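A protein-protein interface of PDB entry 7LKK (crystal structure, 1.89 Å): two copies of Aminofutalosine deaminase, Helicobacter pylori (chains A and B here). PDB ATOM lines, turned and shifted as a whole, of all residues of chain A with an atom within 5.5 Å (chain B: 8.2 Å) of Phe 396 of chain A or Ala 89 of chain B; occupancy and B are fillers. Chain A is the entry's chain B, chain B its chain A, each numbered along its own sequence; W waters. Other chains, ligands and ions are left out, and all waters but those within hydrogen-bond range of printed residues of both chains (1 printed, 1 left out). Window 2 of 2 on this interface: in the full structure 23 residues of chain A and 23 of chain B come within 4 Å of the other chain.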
ATOM      1  N   LEU A  23      35.850  -8.613  32.832  1.00  0.00           N
ATOM      2  CA  LEU A  23      35.280  -9.940  32.665  1.00  0.00           C
ATOM      3  C   LEU A  23      36.392 -10.973  32.747  1.00  0.00           C
ATOM      4  O   LEU A  23      37.459 -10.794  32.153  1.00  0.00           O
ATOM      5  CB  LEU A  23      34.543 -10.070  31.324  1.00  0.00           C
ATOM      6  CG  LEU A  23      33.267  -9.247  31.131  1.00  0.00           C
ATOM      7  CD1 LEU A  23      32.915  -9.148  29.652  1.00  0.00           C
ATOM      8  CD2 LEU A  23      32.117  -9.853  31.914  1.00  0.00           C
ATOM      9  N   VAL A  70      38.768  -8.821  28.746  1.00  0.00           N
ATOM     10  CA  VAL A  70      38.459 -10.189  29.141  1.00  0.00           C
ATOM     11  C   VAL A  70      39.757 -10.873  29.542  1.00  0.00           C
ATOM     12  O   VAL A  70      40.728 -10.869  28.776  1.00  0.00           O
ATOM     13  CB  VAL A  70      37.760 -10.972  28.015  1.00  0.00           C
ATOM     14  CG1 VAL A  70      37.658 -12.446  28.385  1.00  0.00           C
ATOM     15  CG2 VAL A  70      36.385 -10.394  27.737  1.00  0.00           C
ATOM     16  N   PHE A 392      38.812  -4.446  24.667  1.00  0.00           N
ATOM     17  CA  PHE A 392      37.705  -4.055  23.808  1.00  0.00           C
ATOM     18  C   PHE A 392      37.311  -2.613  24.100  1.00  0.00           C
ATOM     19  O   PHE A 392      37.828  -1.974  25.020  1.00  0.00           O
ATOM     20  CB  PHE A 392      36.497  -4.985  24.000  1.00  0.00           C
ATOM     21  CG  PHE A 392      36.802  -6.436  23.742  1.00  0.00           C
ATOM     22  CD1 PHE A 392      36.822  -6.933  22.449  1.00  0.00           C
ATOM     23  CD2 PHE A 392      37.075  -7.298  24.791  1.00  0.00           C
ATOM     24  CE1 PHE A 392      37.102  -8.267  22.210  1.00  0.00           C
ATOM     25  CE2 PHE A 392      37.355  -8.630  24.556  1.00  0.00           C
ATOM     26  CZ  PHE A 392      37.370  -9.114  23.265  1.00  0.00           C
ATOM     27  N   GLU A 394      34.102  -1.774  24.756  1.00  0.00           N
ATOM     28  CA  GLU A 394      32.911  -1.788  25.588  1.00  0.00           C
ATOM     29  C   GLU A 394      32.972  -3.004  26.498  1.00  0.00           C
ATOM     30  O   GLU A 394      33.764  -3.927  26.283  1.00  0.00           O
ATOM     31  CB  GLU A 394      31.629  -1.812  24.744  1.00  0.00           C
ATOM     32  N   LYS A 395      32.135  -2.991  27.529  1.00  0.00           N
ATOM     33  CA  LYS A 395      32.017  -4.112  28.453  1.00  0.00           C
ATOM     34  C   LYS A 395      30.782  -4.926  28.083  1.00  0.00           C
ATOM     35  O   LYS A 395      29.670  -4.391  28.043  1.00  0.00           O
ATOM     36  CB  LYS A 395      31.943  -3.617  29.896  1.00  0.00           C
ATOM     37  CG  LYS A 395      31.945  -4.714  30.944  1.00  0.00           C
ATOM     38  CD  LYS A 395      31.609  -4.183  32.329  1.00  0.00           C
ATOM     39  CE  LYS A 395      32.051  -2.734  32.505  1.00  0.00           C
ATOM     40  NZ  LYS A 395      33.471  -2.636  32.949  1.00  0.00           N
ATOM     41  N   PHE A 396      30.982  -6.211  27.807  1.00  0.00           N
ATOM     42  CA  PHE A 396      29.886  -7.082  27.410  1.00  0.00           C
ATOM     43  C   PHE A 396      29.026  -7.444  28.614  1.00  0.00           C
ATOM     44  O   PHE A 396      29.509  -7.526  29.747  1.00  0.00           O
ATOM     45  CB  PHE A 396      30.414  -8.369  26.772  1.00  0.00           C
ATOM     46  CG  PHE A 396      31.458  -8.152  25.720  1.00  0.00           C
ATOM     47  CD1 PHE A 396      31.365  -7.102  24.828  1.00  0.00           C
ATOM     48  CD2 PHE A 396      32.544  -9.010  25.628  1.00  0.00           C
ATOM     49  CE1 PHE A 396      32.335  -6.909  23.858  1.00  0.00           C
ATOM     50  CE2 PHE A 396      33.515  -8.822  24.659  1.00  0.00           C
ATOM     51  CZ  PHE A 396      33.409  -7.770  23.775  1.00  0.00           C
ATOM     52  N   THR A 397      27.738  -7.665  28.356  1.00  0.00           N
ATOM     53  CA  THR A 397      26.875  -8.241  29.374  1.00  0.00           C
ATOM     54  C   THR A 397      27.328  -9.660  29.703  1.00  0.00           C
ATOM     55  O   THR A 397      27.976 -10.338  28.900  1.00  0.00           O
ATOM     56  CB  THR A 397      25.415  -8.245  28.918  1.00  0.00           C
ATOM     57  OG1 THR A 397      25.250  -9.178  27.845  1.00  0.00           O
ATOM     58  CG2 THR A 397      25.000  -6.858  28.450  1.00  0.00           C
ATOM     59  N   LYS A 398      26.982 -10.098  30.914  1.00  0.00           N
ATOM     60  CA  LYS A 398      27.386 -11.420  31.386  1.00  0.00           C
ATOM     61  C   LYS A 398      26.929 -12.519  30.434  1.00  0.00           C
ATOM     62  O   LYS A 398      27.700 -13.423  30.093  1.00  0.00           O
ATOM     63  CB  LYS A 398      26.823 -11.657  32.788  1.00  0.00           C
ATOM     64  CG  LYS A 398      27.671 -12.548  33.673  1.00  0.00           C
ATOM     65  CD  LYS A 398      27.028 -12.700  35.045  1.00  0.00           C
ATOM     66  CE  LYS A 398      27.987 -13.306  36.051  1.00  0.00           C
ATOM     67  NZ  LYS A 398      27.421 -13.304  37.428  1.00  0.00           N
ATOM     68  N   GLN A 400      26.144 -12.301  27.267  1.00  0.00           N
ATOM     69  CA  GLN A 400      26.692 -12.153  25.927  1.00  0.00           C
ATOM     70  C   GLN A 400      28.212 -12.217  25.895  1.00  0.00           C
ATOM     71  O   GLN A 400      28.787 -12.246  24.802  1.00  0.00           O
ATOM     72  CB  GLN A 400      26.233 -10.825  25.308  1.00  0.00           C
ATOM     73  CG  GLN A 400      24.745 -10.753  24.997  1.00  0.00           C
ATOM     74  CD  GLN A 400      24.400 -11.385  23.666  1.00  0.00           C
ATOM     75  OE1 GLN A 400      25.064 -11.140  22.660  1.00  0.00           O
ATOM     76  NE2 GLN A 400      23.352 -12.200  23.651  1.00  0.00           N
ATOM     77  N   ALA A 401      28.867 -12.266  27.059  1.00  0.00           N
ATOM     78  CA  ALA A 401      30.307 -12.040  27.123  1.00  0.00           C
ATOM     79  C   ALA A 401      31.079 -13.041  26.267  1.00  0.00           C
ATOM     80  O   ALA A 401      31.975 -12.658  25.507  1.00  0.00           O
ATOM     81  CB  ALA A 401      30.781 -12.096  28.575  1.00  0.00           C
ATOM     82  N   GLN A 404      30.302 -12.549  22.353  1.00  0.00           N
ATOM     83  CA  GLN A 404      30.872 -11.295  21.873  1.00  0.00           C
ATOM     84  C   GLN A 404      32.394 -11.345  21.875  1.00  0.00           C
ATOM     85  O   GLN A 404      33.041 -10.770  20.993  1.00  0.00           O
ATOM     86  CB  GLN A 404      30.372 -10.124  22.723  1.00  0.00           C
ATOM     87  CG  GLN A 404      28.863  -9.912  22.678  1.00  0.00           C
ATOM     88  CD  GLN A 404      28.388  -9.275  21.385  1.00  0.00           C
ATOM     89  OE1 GLN A 404      29.178  -8.714  20.626  1.00  0.00           O
ATOM     90  NE2 GLN A 404      27.085  -9.348  21.134  1.00  0.00           N
ATOM     91  N   PHE A 405      32.984 -12.014  22.868  1.00  0.00           N
ATOM     92  CA  PHE A 405      34.432 -12.196  22.882  1.00  0.00           C
ATOM     93  C   PHE A 405      34.899 -12.941  21.636  1.00  0.00           C
ATOM     94  O   PHE A 405      35.827 -12.504  20.949  1.00  0.00           O
ATOM     95  CB  PHE A 405      34.858 -12.941  24.148  1.00  0.00           C
ATOM     96  CG  PHE A 405      36.270 -13.452  24.103  1.00  0.00           C
ATOM     97  CD1 PHE A 405      37.329 -12.617  24.416  1.00  0.00           C
ATOM     98  CD2 PHE A 405      36.538 -14.764  23.752  1.00  0.00           C
ATOM     99  CE1 PHE A 405      38.628 -13.082  24.378  1.00  0.00           C
ATOM    100  CE2 PHE A 405      37.839 -15.236  23.710  1.00  0.00           C
ATOM    101  CZ  PHE A 405      38.885 -14.395  24.022  1.00  0.00           C
ATOM    102  N   HIS A 408      34.650 -10.697  18.421  1.00  0.00           N
ATOM    103  CA  HIS A 408      35.444  -9.486  18.279  1.00  0.00           C
ATOM    104  C   HIS A 408      36.919  -9.640  18.624  1.00  0.00           C
ATOM    105  O   HIS A 408      37.711  -8.775  18.237  1.00  0.00           O
ATOM    106  CB  HIS A 408      34.847  -8.365  19.144  1.00  0.00           C
ATOM    107  CG  HIS A 408      33.430  -8.034  18.793  1.00  0.00           C
ATOM    108  ND1 HIS A 408      33.074  -7.495  17.576  1.00  0.00           N
ATOM    109  CD2 HIS A 408      32.279  -8.182  19.490  1.00  0.00           C
ATOM    110  CE1 HIS A 408      31.765  -7.318  17.541  1.00  0.00           C
ATOM    111  NE2 HIS A 408      31.259  -7.726  18.691  1.00  0.00           N
ATOM    112  N   ASN B  86      28.854   2.318  13.686  1.00  0.00           N
ATOM    113  CA  ASN B  86      29.517   2.430  14.981  1.00  0.00           C
ATOM    114  C   ASN B  86      29.489   1.129  15.770  1.00  0.00           C
ATOM    115  O   ASN B  86      30.306   0.955  16.682  1.00  0.00           O
ATOM    116  CB  ASN B  86      28.865   3.531  15.820  1.00  0.00           C
ATOM    117  CG  ASN B  86      29.495   4.890  15.600  1.00  0.00           C
ATOM    118  OD1 ASN B  86      30.663   4.994  15.226  1.00  0.00           O
ATOM    119  ND2 ASN B  86      28.723   5.945  15.843  1.00  0.00           N
ATOM    120  N   ASN B  87      28.579   0.216  15.439  1.00  0.00           N
ATOM    121  CA  ASN B  87      28.281  -0.903  16.319  1.00  0.00           C
ATOM    122  C   ASN B  87      29.434  -1.895  16.405  1.00  0.00           C
ATOM    123  O   ASN B  87      30.040  -2.266  15.397  1.00  0.00           O
ATOM    124  CB  ASN B  87      27.025  -1.632  15.850  1.00  0.00           C
ATOM    125  CG  ASN B  87      26.659  -2.789  16.758  1.00  0.00           C
ATOM    126  OD1 ASN B  87      26.591  -2.633  17.976  1.00  0.00           O
ATOM    127  ND2 ASN B  87      26.444  -3.961  16.173  1.00  0.00           N
ATOM    128  N   LYS B  88      29.727  -2.324  17.635  1.00  0.00           N
ATOM    129  CA  LYS B  88      30.548  -3.510  17.875  1.00  0.00           C
ATOM    130  C   LYS B  88      29.784  -4.503  18.739  1.00  0.00           C
ATOM    131  O   LYS B  88      29.437  -5.584  18.259  1.00  0.00           O
ATOM    132  CB  LYS B  88      31.885  -3.125  18.513  1.00  0.00           C
ATOM    133  CG  LYS B  88      32.664  -2.074  17.742  1.00  0.00           C
ATOM    134  CD  LYS B  88      33.838  -2.690  17.001  1.00  0.00           C
ATOM    135  CE  LYS B  88      34.719  -1.618  16.383  1.00  0.00           C
ATOM    136  NZ  LYS B  88      33.935  -0.686  15.532  1.00  0.00           N
ATOM    137  N   ALA B  89      29.487  -4.165  19.997  1.00  0.00           N
ATOM    138  CA  ALA B  89      28.768  -5.057  20.899  1.00  0.00           C
ATOM    139  C   ALA B  89      27.558  -4.371  21.524  1.00  0.00           C
ATOM    140  O   ALA B  89      27.118  -4.750  22.613  1.00  0.00           O
ATOM    141  CB  ALA B  89      29.696  -5.591  21.988  1.00  0.00           C
ATOM    142  N   SER B  90      27.006  -3.355  20.856  1.00  0.00           N
ATOM    143  CA  SER B  90      25.835  -2.671  21.396  1.00  0.00           C
ATOM    144  C   SER B  90      24.574  -3.520  21.311  1.00  0.00           C
ATOM    145  O   SER B  90      23.634  -3.288  22.081  1.00  0.00           O
ATOM    146  CB  SER B  90      25.610  -1.342  20.669  1.00  0.00           C
ATOM    147  OG  SER B  90      26.708  -0.463  20.848  1.00  0.00           O
ATOM    148  N   PHE B  91      24.531  -4.498  20.410  1.00  0.00           N
ATOM    149  CA  PHE B  91      23.340  -5.298  20.170  1.00  0.00           C
ATOM    150  C   PHE B  91      23.594  -6.751  20.550  1.00  0.00           C
ATOM    151  O   PHE B  91      24.709  -7.262  20.408  1.00  0.00           O
ATOM    152  CB  PHE B  91      22.897  -5.215  18.699  1.00  0.00           C
ATOM    153  CG  PHE B  91      22.709  -3.809  18.193  1.00  0.00           C
ATOM    154  CD1 PHE B  91      22.193  -2.821  19.017  1.00  0.00           C
ATOM    155  CD2 PHE B  91      23.037  -3.479  16.889  1.00  0.00           C
ATOM    156  CE1 PHE B  91      22.018  -1.527  18.550  1.00  0.00           C
ATOM    157  CE2 PHE B  91      22.864  -2.188  16.416  1.00  0.00           C
ATOM    158  CZ  PHE B  91      22.353  -1.212  17.249  1.00  0.00           C
ATOM    159  N   ASP B  92      22.552  -7.408  21.051  1.00  0.00           N
ATOM    160  CA  ASP B  92      22.644  -8.805  21.448  1.00  0.00           C
ATOM    161  C   ASP B  92      22.562  -9.724  20.233  1.00  0.00           C
ATOM    162  O   ASP B  92      21.859  -9.442  19.260  1.00  0.00           O
ATOM    163  CB  ASP B  92      21.530  -9.165  22.430  1.00  0.00           C
ATOM    164  CG  ASP B  92      21.673  -8.462  23.767  1.00  0.00           C
ATOM    165  OD1 ASP B  92      22.754  -7.900  24.044  1.00  0.00           O
ATOM    166  OD2 ASP B  92      20.696  -8.475  24.543  1.00  0.00           O
ATOM    167  N   TYR B  93      23.289 -10.834  20.303  1.00  0.00           N
ATOM    168  CA  TYR B  93      23.261 -11.862  19.274  1.00  0.00           C
ATOM    169  C   TYR B  93      22.826 -13.187  19.887  1.00  0.00           C
ATOM    170  O   TYR B  93      22.813 -13.357  21.109  1.00  0.00           O
ATOM    171  CB  TYR B  93      24.632 -12.011  18.596  1.00  0.00           C
ATOM    172  CG  TYR B  93      25.073 -10.773  17.847  1.00  0.00           C
ATOM    173  CD1 TYR B  93      24.202 -10.105  16.994  1.00  0.00           C
ATOM    174  CD2 TYR B  93      26.356 -10.266  17.999  1.00  0.00           C
ATOM    175  CE1 TYR B  93      24.598  -8.970  16.309  1.00  0.00           C
ATOM    176  CE2 TYR B  93      26.764  -9.133  17.318  1.00  0.00           C
ATOM    177  CZ  TYR B  93      25.880  -8.491  16.473  1.00  0.00           C
ATOM    178  OH  TYR B  93      26.280  -7.364  15.794  1.00  0.00           O
ATOM    179  N   SER B 102      17.292  -5.388  21.602  1.00  0.00           N
ATOM    180  CA  SER B 102      18.455  -4.602  22.002  1.00  0.00           C
ATOM    181  C   SER B 102      18.651  -3.390  21.099  1.00  0.00           C
ATOM    182  O   SER B 102      19.095  -2.337  21.569  1.00  0.00           O
ATOM    183  CB  SER B 102      19.714  -5.475  22.014  1.00  0.00           C
ATOM    184  OG  SER B 102      20.161  -5.758  20.699  1.00  0.00           O
ATOM    185  N   ASN B 106      18.419   0.369  22.530  1.00  0.00           N
ATOM    186  CA  ASN B 106      19.554   1.268  22.345  1.00  0.00           C
ATOM    187  C   ASN B 106      19.101   2.706  22.127  1.00  0.00           C
ATOM    188  O   ASN B 106      19.838   3.644  22.451  1.00  0.00           O
ATOM    189  CB  ASN B 106      20.409   0.791  21.169  1.00  0.00           C
ATOM    190  CG  ASN B 106      21.571   1.720  20.876  1.00  0.00           C
ATOM    191  OD1 ASN B 106      21.464   2.626  20.047  1.00  0.00           O
ATOM    192  ND2 ASN B 106      22.692   1.497  21.553  1.00  0.00           N
ATOM    193  N   ILE B 110      23.657   4.593  19.222  1.00  0.00           N
ATOM    194  CA  ILE B 110      24.770   4.150  18.392  1.00  0.00           C
ATOM    195  C   ILE B 110      24.851   4.944  17.095  1.00  0.00           C
ATOM    196  O   ILE B 110      25.906   4.970  16.451  1.00  0.00           O
ATOM    197  CB  ILE B 110      24.653   2.637  18.114  1.00  0.00           C
ATOM    198  CG1 ILE B 110      25.994   2.059  17.651  1.00  0.00           C
ATOM    199  CG2 ILE B 110      23.561   2.356  17.092  1.00  0.00           C
ATOM    200  CD1 ILE B 110      27.080   2.110  18.702  1.00  0.00           C
ATOM    201  N   LEU B 330      27.180  -3.379  10.110  1.00  0.00           N
ATOM    202  CA  LEU B 330      27.877  -3.748  11.336  1.00  0.00           C
ATOM    203  C   LEU B 330      26.930  -3.871  12.523  1.00  0.00           C
ATOM    204  O   LEU B 330      27.362  -4.292  13.599  1.00  0.00           O
ATOM    205  CB  LEU B 330      28.981  -2.735  11.644  1.00  0.00           C
ATOM    206  CG  LEU B 330      30.183  -2.773  10.696  1.00  0.00           C
ATOM    207  CD1 LEU B 330      31.208  -1.707  11.059  1.00  0.00           C
ATOM    208  CD2 LEU B 330      30.823  -4.156  10.695  1.00  0.00           C
ATOM    209  N   SER B 331      25.660  -3.494  12.354  1.00  0.00           N
ATOM    210  CA  SER B 331      24.643  -3.810  13.348  1.00  0.00           C
ATOM    211  C   SER B 331      24.406  -5.309  13.468  1.00  0.00           C
ATOM    212  O   SER B 331      23.840  -5.758  14.471  1.00  0.00           O
ATOM    213  CB  SER B 331      23.332  -3.102  12.998  1.00  0.00           C
ATOM    214  OG  SER B 331      23.130  -3.069  11.595  1.00  0.00           O
ATOM    215  N   ASN B 333      27.003  -7.752  11.972  1.00  0.00           N
ATOM    216  CA  ASN B 333      28.183  -8.341  11.351  1.00  0.00           C
ATOM    217  C   ASN B 333      29.410  -7.808  12.074  1.00  0.00           C
ATOM    218  O   ASN B 333      29.341  -6.824  12.815  1.00  0.00           O
ATOM    219  CB  ASN B 333      28.247  -8.025   9.851  1.00  0.00           C
ATOM    220  CG  ASN B 333      28.926  -9.121   9.044  1.00  0.00           C
ATOM    221  OD1 ASN B 333      29.868  -9.765   9.508  1.00  0.00           O
ATOM    222  ND2 ASN B 333      28.445  -9.333   7.822  1.00  0.00           N
HETATM  223  O   HOH W   1      28.148  -4.526  25.425  1.00  0.00           O
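No position is printed for both chains.
Of the 13 printed residues of chain A, 4 touch a printed residue of chain B. Along chain A the printed residues that touch a printed residue of chain B span positions 396 to 408. Printed residues of chain B that touch a printed residue of chain A: Lys 88, Ala 89, Phe 91, Asp 92 and Tyr 93.
The side-chain amide nitrogen of Asn 87 of chain B lies within hydrogen-bond range of the side-chain hydroxyl of Tyr 93 of chain B (3.4 Å). The backbone NH (N) of Asp 92 of chain B lies within hydrogen-bond range of the side-chain hydroxyl (OG) of Ser 102 of chain B, 2.9 Å away. The side-chain hydroxyl (OH) of Tyr 93 of chain B is in hydrogen-bond range of the backbone carbonyl oxygen (O) of Ser 331 of chain B, 3.2 Å away. The backbone NH (N) of Gln 400 of chain A lies close to the side-chain hydroxyl (OG1) of Thr 397 of chain A, 3.3 Å away. OE1 of Gln 400 of chain A sits at hydrogen-bond distance from NE2 of Gln 404 of chain A (3.1 Å). NE2 of His 408 of chain A sits at hydrogen-bond distance from OE1 of Gln 404 of chain A (3.0 Å).
Glu 394 of chain A touches none of the printed residues of chain B. Phe 396 of chain A touches one residue of chain B. Of chain A, only Phe 396 and Gln 404 come within 4 Å of Ala 89 of chain B. Of the printed residues of chain A, Phe 91 of chain B touches Gln 404. Of the printed residues of chain A, Asp 92 of chain B touches Gln 400 (3.6 Å). Ser 102 of chain B touches none of the printed residues of chain A. The nearest residue of chain B that does not touch Phe 396 of chain A is Lys 88 of chain B (6.2 Å). The nearest residue of chain A that does not touch Ala 89 of chain B is His 408 of chain A (4.2 Å). The nearest printed residue of chain A that does not touch Lys 88 of chain B is Phe 396 of chain A (6.2 Å).
Ala 89 of chain B touches Phe 396 of chain A. Gln 400 of chain A touches Asp 92 of chain B. Gln 404 of chain A touches Lys 88 of chain B. Ala 89 of chain B touches Gln 404 of chain A. Tyr 93 of chain B touches Gln 404 of chain A.
NE2 of His 408 of chain A lies within hydrogen-bond range of O of Lys 88 of chain B, 2.8 Å away. The backbone carbonyl oxygen (O) of Phe 91 of chain B is in hydrogen-bond range of the side-chain amide nitrogen (NE2) of Gln 404 of chain A (3.2 Å). O of Tyr 93 of chain B is in hydrogen-bond range of NE2 of Gln 400 of chain A (2.8 Å).
Water W1 bridges O of Ala 89 of chain B (3.0 Å) and O of Lys 395 of chain A (3.0 Å).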
